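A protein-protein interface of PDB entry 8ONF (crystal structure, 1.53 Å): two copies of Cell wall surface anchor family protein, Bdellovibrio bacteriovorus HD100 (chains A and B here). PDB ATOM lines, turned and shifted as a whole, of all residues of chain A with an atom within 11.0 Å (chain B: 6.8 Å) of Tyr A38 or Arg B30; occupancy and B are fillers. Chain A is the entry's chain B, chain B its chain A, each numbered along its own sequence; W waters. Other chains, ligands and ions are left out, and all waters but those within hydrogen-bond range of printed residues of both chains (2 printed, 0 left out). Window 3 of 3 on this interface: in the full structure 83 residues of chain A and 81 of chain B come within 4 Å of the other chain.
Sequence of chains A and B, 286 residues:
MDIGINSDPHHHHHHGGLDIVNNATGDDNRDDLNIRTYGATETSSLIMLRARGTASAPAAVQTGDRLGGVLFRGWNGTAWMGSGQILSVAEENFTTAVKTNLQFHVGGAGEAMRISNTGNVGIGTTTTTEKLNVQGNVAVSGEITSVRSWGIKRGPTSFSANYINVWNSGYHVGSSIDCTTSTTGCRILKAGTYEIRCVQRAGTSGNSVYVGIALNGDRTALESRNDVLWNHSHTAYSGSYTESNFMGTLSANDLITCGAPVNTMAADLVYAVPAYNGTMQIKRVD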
ATOM      1  N   LEU A  33     -26.424   6.682 -17.458  1.00  0.00           N
ATOM      2  CA  LEU A  33     -27.435   6.081 -16.603  1.00  0.00           C
ATOM      3  C   LEU A  33     -27.015   4.650 -16.311  1.00  0.00           C
ATOM      4  O   LEU A  33     -26.830   3.858 -17.239  1.00  0.00           O
ATOM      5  CB  LEU A  33     -28.799   6.105 -17.285  1.00  0.00           C
ATOM      6  CG  LEU A  33     -29.186   7.411 -17.968  1.00  0.00           C
ATOM      7  CD1 LEU A  33     -30.692   7.507 -18.068  1.00  0.00           C
ATOM      8  CD2 LEU A  33     -28.629   8.587 -17.177  1.00  0.00           C
ATOM      9  N   ASN A  34     -26.860   4.319 -15.032  1.00  0.00           N
ATOM     10  CA  ASN A  34     -26.470   2.981 -14.611  1.00  0.00           C
ATOM     11  C   ASN A  34     -27.615   2.309 -13.874  1.00  0.00           C
ATOM     12  O   ASN A  34     -28.314   2.940 -13.076  1.00  0.00           O
ATOM     13  CB  ASN A  34     -25.236   3.004 -13.712  1.00  0.00           C
ATOM     14  CG  ASN A  34     -24.048   3.659 -14.377  1.00  0.00           C
ATOM     15  OD1 ASN A  34     -23.331   3.027 -15.149  1.00  0.00           O
ATOM     16  ND2 ASN A  34     -23.834   4.934 -14.080  1.00  0.00           N
ATOM     17  N   ILE A  35     -27.810   1.027 -14.162  1.00  0.00           N
ATOM     18  CA  ILE A  35     -28.714   0.170 -13.410  1.00  0.00           C
ATOM     19  C   ILE A  35     -27.911  -1.045 -12.979  1.00  0.00           C
ATOM     20  O   ILE A  35     -27.426  -1.803 -13.827  1.00  0.00           O
ATOM     21  CB  ILE A  35     -29.942  -0.259 -14.223  1.00  0.00           C
ATOM     22  CG1 ILE A  35     -30.578   0.946 -14.924  1.00  0.00           C
ATOM     23  CG2 ILE A  35     -30.947  -0.958 -13.310  1.00  0.00           C
ATOM     24  CD1 ILE A  35     -31.780   0.574 -15.780  1.00  0.00           C
ATOM     25  N   ARG A  36     -27.767  -1.225 -11.673  1.00  0.00           N
ATOM     26  CA  ARG A  36     -26.917  -2.256 -11.091  1.00  0.00           C
ATOM     27  C   ARG A  36     -27.779  -3.173 -10.246  1.00  0.00           C
ATOM     28  O   ARG A  36     -28.548  -2.701  -9.402  1.00  0.00           O
ATOM     29  CB  ARG A  36     -25.834  -1.645 -10.203  1.00  0.00           C
ATOM     30  CG  ARG A  36     -24.720  -2.593  -9.801  1.00  0.00           C
ATOM     31  CD  ARG A  36     -23.687  -1.837  -8.975  1.00  0.00           C
ATOM     32  NE  ARG A  36     -22.792  -1.045  -9.812  1.00  0.00           N
ATOM     33  CZ  ARG A  36     -21.485  -0.928  -9.614  1.00  0.00           C
ATOM     34  NH1 ARG A  36     -20.881  -1.541  -8.608  1.00  0.00           N
ATOM     35  NH2 ARG A  36     -20.771  -0.169 -10.439  1.00  0.00           N
ATOM     36  N   THR A  37     -27.635  -4.476 -10.447  1.00  0.00           N
ATOM     37  CA  THR A  37     -28.372  -5.451  -9.661  1.00  0.00           C
ATOM     38  C   THR A  37     -27.419  -6.521  -9.162  1.00  0.00           C
ATOM     39  O   THR A  37     -26.596  -7.046  -9.924  1.00  0.00           O
ATOM     40  CB  THR A  37     -29.520  -6.074 -10.471  1.00  0.00           C
ATOM     41  OG1 THR A  37     -30.353  -5.033 -11.004  1.00  0.00           O
ATOM     42  CG2 THR A  37     -30.336  -7.033  -9.610  1.00  0.00           C
ATOM     43  N   TYR A  38     -27.522  -6.817  -7.877  1.00  0.00           N
ATOM     44  CA  TYR A  38     -26.812  -7.917  -7.264  1.00  0.00           C
ATOM     45  C   TYR A  38     -27.802  -9.024  -6.933  1.00  0.00           C
ATOM     46  O   TYR A  38     -29.024  -8.863  -7.028  1.00  0.00           O
ATOM     47  CB  TYR A  38     -26.081  -7.455  -5.998  1.00  0.00           C
ATOM     48  CG  TYR A  38     -24.962  -6.469  -6.239  1.00  0.00           C
ATOM     49  CD1 TYR A  38     -25.215  -5.101  -6.321  1.00  0.00           C
ATOM     50  CD2 TYR A  38     -23.653  -6.908  -6.408  1.00  0.00           C
ATOM     51  CE1 TYR A  38     -24.187  -4.196  -6.533  1.00  0.00           C
ATOM     52  CE2 TYR A  38     -22.626  -6.020  -6.625  1.00  0.00           C
ATOM     53  CZ  TYR A  38     -22.894  -4.666  -6.696  1.00  0.00           C
ATOM     54  OH  TYR A  38     -21.861  -3.786  -6.907  1.00  0.00           O
ATOM     55  N   GLY A  39     -27.269 -10.161  -6.551  1.00  0.00           N
ATOM     56  CA  GLY A  39     -28.090 -11.207  -5.979  1.00  0.00           C
ATOM     57  C   GLY A  39     -28.406 -12.332  -6.946  1.00  0.00           C
ATOM     58  O   GLY A  39     -28.008 -12.352  -8.116  1.00  0.00           O
ATOM     59  N   ALA A  40     -29.197 -13.255  -6.408  1.00  0.00           N
ATOM     60  CA  ALA A  40     -29.417 -14.571  -6.989  1.00  0.00           C
ATOM     61  C   ALA A  40     -30.562 -14.622  -7.987  1.00  0.00           C
ATOM     62  O   ALA A  40     -30.582 -15.529  -8.824  1.00  0.00           O
ATOM     63  CB  ALA A  40     -29.697 -15.583  -5.875  1.00  0.00           C
ATOM     64  N   THR A  41     -31.507 -13.685  -7.938  1.00  0.00           N
ATOM     65  CA  THR A  41     -32.744 -13.848  -8.694  1.00  0.00           C
ATOM     66  C   THR A  41     -33.170 -12.647  -9.537  1.00  0.00           C
ATOM     67  O   THR A  41     -33.962 -12.842 -10.469  1.00  0.00           O
ATOM     68  CB  THR A  41     -33.905 -14.200  -7.747  1.00  0.00           C
ATOM     69  OG1 THR A  41     -33.972 -13.218  -6.714  1.00  0.00           O
ATOM     70  CG2 THR A  41     -33.678 -15.561  -7.093  1.00  0.00           C
ATOM     71  N   GLU A  42     -32.707 -11.431  -9.252  1.00  0.00           N
ATOM     72  CA  GLU A  42     -33.234 -10.243  -9.921  1.00  0.00           C
ATOM     73  C   GLU A  42     -32.280  -9.736 -11.002  1.00  0.00           C
ATOM     74  O   GLU A  42     -31.120 -10.156 -11.099  1.00  0.00           O
ATOM     75  CB  GLU A  42     -33.512  -9.127  -8.902  1.00  0.00           C
ATOM     76  CG  GLU A  42     -34.414  -9.536  -7.730  1.00  0.00           C
ATOM     77  CD  GLU A  42     -35.879  -9.639  -8.097  1.00  0.00           C
ATOM     78  OE1 GLU A  42     -36.233  -9.348  -9.266  1.00  0.00           O
ATOM     79  OE2 GLU A  42     -36.684 -10.019  -7.214  1.00  0.00           O
ATOM     80  N   THR A  43     -32.782  -8.798 -11.813  1.00  0.00           N
ATOM     81  CA  THR A  43     -32.004  -8.270 -12.928  1.00  0.00           C
ATOM     82  C   THR A  43     -32.314  -6.789 -13.114  1.00  0.00           C
ATOM     83  O   THR A  43     -33.301  -6.264 -12.590  1.00  0.00           O
ATOM     84  CB  THR A  43     -32.283  -9.040 -14.233  1.00  0.00           C
ATOM     85  OG1 THR A  43     -31.407  -8.578 -15.276  1.00  0.00           O
ATOM     86  CG2 THR A  43     -33.739  -8.835 -14.667  1.00  0.00           C
ATOM     87  N   SER A  44     -31.453  -6.125 -13.878  1.00  0.00           N
ATOM     88  CA  SER A  44     -31.604  -4.706 -14.181  1.00  0.00           C
ATOM     89  C   SER A  44     -32.501  -4.520 -15.404  1.00  0.00           C
ATOM     90  O   SER A  44     -32.254  -5.130 -16.451  1.00  0.00           O
ATOM     91  CB  SER A  44     -30.230  -4.082 -14.441  1.00  0.00           C
ATOM     92  OG  SER A  44     -29.397  -4.152 -13.290  1.00  0.00           O
ATOM     93  N   SER A  45     -33.523  -3.662 -15.290  1.00  0.00           N
ATOM     94  CA  SER A  45     -34.394  -3.378 -16.430  1.00  0.00           C
ATOM     95  C   SER A  45     -34.632  -1.888 -16.617  1.00  0.00           C
ATOM     96  O   SER A  45     -34.917  -1.171 -15.653  1.00  0.00           O
ATOM     97  CB  SER A  45     -35.760  -4.068 -16.302  1.00  0.00           C
ATOM     98  OG  SER A  45     -35.649  -5.410 -15.890  1.00  0.00           O
ATOM     99  N   LEU A  46     -34.547  -1.439 -17.867  1.00  0.00           N
ATOM    100  CA  LEU A  46     -35.179  -0.198 -18.300  1.00  0.00           C
ATOM    101  C   LEU A  46     -36.550  -0.569 -18.844  1.00  0.00           C
ATOM    102  O   LEU A  46     -36.641  -1.399 -19.752  1.00  0.00           O
ATOM    103  CB  LEU A  46     -34.347   0.490 -19.377  1.00  0.00           C
ATOM    104  CG  LEU A  46     -35.014   1.616 -20.168  1.00  0.00           C
ATOM    105  CD1 LEU A  46     -35.251   2.803 -19.260  1.00  0.00           C
ATOM    106  CD2 LEU A  46     -34.160   2.008 -21.373  1.00  0.00           C
ATOM    107  N   ILE A  47     -37.605   0.023 -18.285  1.00  0.00           N
ATOM    108  CA  ILE A  47     -38.981  -0.311 -18.640  1.00  0.00           C
ATOM    109  C   ILE A  47     -39.666   0.925 -19.202  1.00  0.00           C
ATOM    110  O   ILE A  47     -39.692   1.978 -18.556  1.00  0.00           O
ATOM    111  CB  ILE A  47     -39.763  -0.863 -17.435  1.00  0.00           C
ATOM    112  CG1 ILE A  47     -38.946  -1.953 -16.727  1.00  0.00           C
ATOM    113  CG2 ILE A  47     -41.148  -1.362 -17.875  1.00  0.00           C
ATOM    114  CD1 ILE A  47     -39.621  -2.543 -15.506  1.00  0.00           C
ATOM    115  N   ASN B  29     -26.975   3.265  -8.942  1.00  0.00           N
ATOM    116  CA  ASN B  29     -28.448   3.069  -8.934  1.00  0.00           C
ATOM    117  C   ASN B  29     -28.825   1.590  -9.082  1.00  0.00           C
ATOM    118  O   ASN B  29     -28.342   0.929  -9.993  1.00  0.00           O
ATOM    119  CB  ASN B  29     -29.174   3.886 -10.000  1.00  0.00           C
ATOM    120  CG  ASN B  29     -30.616   3.461 -10.199  1.00  0.00           C
ATOM    121  OD1 ASN B  29     -31.432   3.558  -9.286  1.00  0.00           O
ATOM    122  ND2 ASN B  29     -30.946   2.994 -11.391  1.00  0.00           N
ATOM    123  N   ARG B  30     -29.709   1.105  -8.209  1.00  0.00           N
ATOM    124  CA  ARG B  30     -30.126  -0.321  -8.255  1.00  0.00           C
ATOM    125  C   ARG B  30     -31.575  -0.421  -8.735  1.00  0.00           C
ATOM    126  O   ARG B  30     -32.028  -1.547  -9.000  1.00  0.00           O
ATOM    127  CB  ARG B  30     -30.053  -0.942  -6.859  1.00  0.00           C
ATOM    128  CG  ARG B  30     -28.704  -0.800  -6.170  1.00  0.00           C
ATOM    129  CD  ARG B  30     -27.683  -1.806  -6.659  1.00  0.00           C
ATOM    130  NE  ARG B  30     -26.688  -2.113  -5.641  1.00  0.00           N
ATOM    131  CZ  ARG B  30     -26.955  -2.682  -4.472  1.00  0.00           C
ATOM    132  NH1 ARG B  30     -28.111  -3.291  -4.277  1.00  0.00           N
ATOM    133  NH2 ARG B  30     -26.058  -2.651  -3.502  1.00  0.00           N
ATOM    134  N   ASP B  31     -32.272   0.710  -8.833  1.00  0.00           N
ATOM    135  CA  ASP B  31     -33.717   0.653  -9.177  1.00  0.00           C
ATOM    136  C   ASP B  31     -33.907   0.577 -10.694  1.00  0.00           C
ATOM    137  O   ASP B  31     -33.128   1.220 -11.420  1.00  0.00           O
ATOM    138  CB  ASP B  31     -34.480   1.843  -8.587  1.00  0.00           C
ATOM    139  CG  ASP B  31     -34.294   1.986  -7.087  1.00  0.00           C
ATOM    140  OD1 ASP B  31     -33.143   2.197  -6.657  1.00  0.00           O
ATOM    141  OD2 ASP B  31     -35.301   1.880  -6.362  1.00  0.00           O
ATOM    142  N   ASP B  32     -34.914  -0.177 -11.141  1.00  0.00           N
ATOM    143  CA  ASP B  32     -35.232  -0.208 -12.589  1.00  0.00           C
ATOM    144  C   ASP B  32     -35.639   1.202 -13.015  1.00  0.00           C
ATOM    145  O   ASP B  32     -36.332   1.877 -12.231  1.00  0.00           O
ATOM    146  CB  ASP B  32     -36.355  -1.195 -12.890  1.00  0.00           C
ATOM    147  CG  ASP B  32     -35.933  -2.648 -12.780  1.00  0.00           C
ATOM    148  OD1 ASP B  32     -34.730  -2.895 -12.558  1.00  0.00           O
ATOM    149  OD2 ASP B  32     -36.815  -3.518 -12.905  1.00  0.00           O
ATOM    150  N   TRP B  75     -20.274  -9.268 -13.578  1.00  0.00           N
ATOM    151  CA  TRP B  75     -19.141  -9.560 -12.704  1.00  0.00           C
ATOM    152  C   TRP B  75     -18.574 -10.940 -13.015  1.00  0.00           C
ATOM    153  O   TRP B  75     -19.319 -11.921 -13.087  1.00  0.00           O
ATOM    154  CB  TRP B  75     -19.575  -9.491 -11.238  1.00  0.00           C
ATOM    155  CG  TRP B  75     -18.429  -9.568 -10.252  1.00  0.00           C
ATOM    156  CD1 TRP B  75     -18.134 -10.614  -9.415  1.00  0.00           C
ATOM    157  CD2 TRP B  75     -17.469  -8.543  -9.962  1.00  0.00           C
ATOM    158  NE1 TRP B  75     -17.032 -10.310  -8.645  1.00  0.00           N
ATOM    159  CE2 TRP B  75     -16.613  -9.043  -8.957  1.00  0.00           C
ATOM    160  CE3 TRP B  75     -17.244  -7.253 -10.461  1.00  0.00           C
ATOM    161  CZ2 TRP B  75     -15.542  -8.302  -8.446  1.00  0.00           C
ATOM    162  CZ3 TRP B  75     -16.181  -6.518  -9.953  1.00  0.00           C
ATOM    163  CH2 TRP B  75     -15.345  -7.047  -8.954  1.00  0.00           C
ATOM    164  N   TRP B  80     -15.899  -6.016 -13.718  1.00  0.00           N
ATOM    165  CA  TRP B  80     -17.079  -5.855 -14.557  1.00  0.00           C
ATOM    166  C   TRP B  80     -16.661  -5.995 -16.016  1.00  0.00           C
ATOM    167  O   TRP B  80     -15.855  -5.200 -16.516  1.00  0.00           O
ATOM    168  CB  TRP B  80     -17.728  -4.495 -14.311  1.00  0.00           C
ATOM    169  CG  TRP B  80     -18.243  -4.322 -12.912  1.00  0.00           C
ATOM    170  CD1 TRP B  80     -17.642  -3.623 -11.894  1.00  0.00           C
ATOM    171  CD2 TRP B  80     -19.465  -4.845 -12.373  1.00  0.00           C
ATOM    172  NE1 TRP B  80     -18.416  -3.687 -10.758  1.00  0.00           N
ATOM    173  CE2 TRP B  80     -19.541  -4.429 -11.023  1.00  0.00           C
ATOM    174  CE3 TRP B  80     -20.510  -5.619 -12.903  1.00  0.00           C
ATOM    175  CZ2 TRP B  80     -20.617  -4.770 -10.194  1.00  0.00           C
ATOM    176  CZ3 TRP B  80     -21.572  -5.958 -12.078  1.00  0.00           C
ATOM    177  CH2 TRP B  80     -21.614  -5.531 -10.737  1.00  0.00           C
HETATM  178  O   HOH W   1     -35.736  -5.733 -13.310  1.00  0.00           O
HETATM  179  O   HOH W   2     -29.317  -5.335  -6.069  1.00  0.00           O
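The backbone carbonyl oxygen of Asn A34 is in hydrogen-bond range of the side-chain amide nitrogen of Asn B29, 3.1 Å away.
The backbone carbonyl oxygen (O) of Asn B29 sits at hydrogen-bond distance from the backbone NH (N) of Arg A36 (2.8 Å).
The backbone NH of Ser A45 lies within hydrogen-bond range of the side-chain carboxylate of Asp B32 (3.1 Å).
O of Asp B31 is in hydrogen-bond range of ND2 of Asn B29, 2.8 Å away.
O of Ile A35 lies within hydrogen-bond range of OG of Ser A44 (3.1 Å).
The guanidinium group (NH1) of Arg A36 is in hydrogen-bond range of the side-chain hydroxyl (OH) of Tyr A38, 3.0 Å away.
OG of Ser A44 sits at hydrogen-bond distance from OG1 of Thr A37, 2.6 Å away.
Water W1 lies within hydrogen-bond range of OD2 of Asp B32, O of Thr A43 and OG of Ser A45.
Water W2 bridges the backbone NH (N) of Tyr A38 and the guanidinium group (NH1) of Arg B30.
Of the 6 printed residues of chain B, 5 touch a printed residue of chain A.
Printed residues of chain B that touch a printed residue of chain A: Asn B29, Arg B30, Asp B31, Asp B32 and Trp B80.
Hydrophobic or aromatic side chains of chain B that line the printed part of chain A: Trp B80.
Among the printed residues, 12 pairs touch across the chains.
No position is printed for both chains.
Of the 12 pairs that touch across the chains among the printed residues, none has its exchanged pair printed and touching as well.
Of the printed residues of chain B, Ile A35 touches Asn B29 (3.5 Å) and Asp B31 (3.6 Å).
Tyr A38 touches just these residues of chain B: Arg B30 and Trp B80.
Printed residues of chain B within 4 Å of Thr A43: Asp B32.
Printed residues of chain B within 4 Å of Ser A44: Asp B32 (3.96 Å).
Asn B29 touches just these residues of chain A: Asn A34 (3.1 Å), Ile A35 (3.5 Å) and Arg A36 (2.8 Å).
Arg B30 touches two residues of chain A.
Asp B32 touches four residues of chain A.
Of the printed residues of chain A, Trp B80 touches Arg A36 (3.6 Å) and Tyr A38 (3.6 Å).
The nearest residue of chain B that does not touch Tyr A38 is Trp B75 (6.5 Å).
Among the printed residues, pairs that only touch across the chains: Arg A36 with Arg B30, Tyr A38 with Arg B30, Ile A35 with Asn B29, Arg A36 with Trp B80, Ile A35 with Asp B31, Tyr A38 with Trp B80, Thr A43 with Asp B32, Ile A47 with Asp B32 and Ser A44 with Asp B32.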
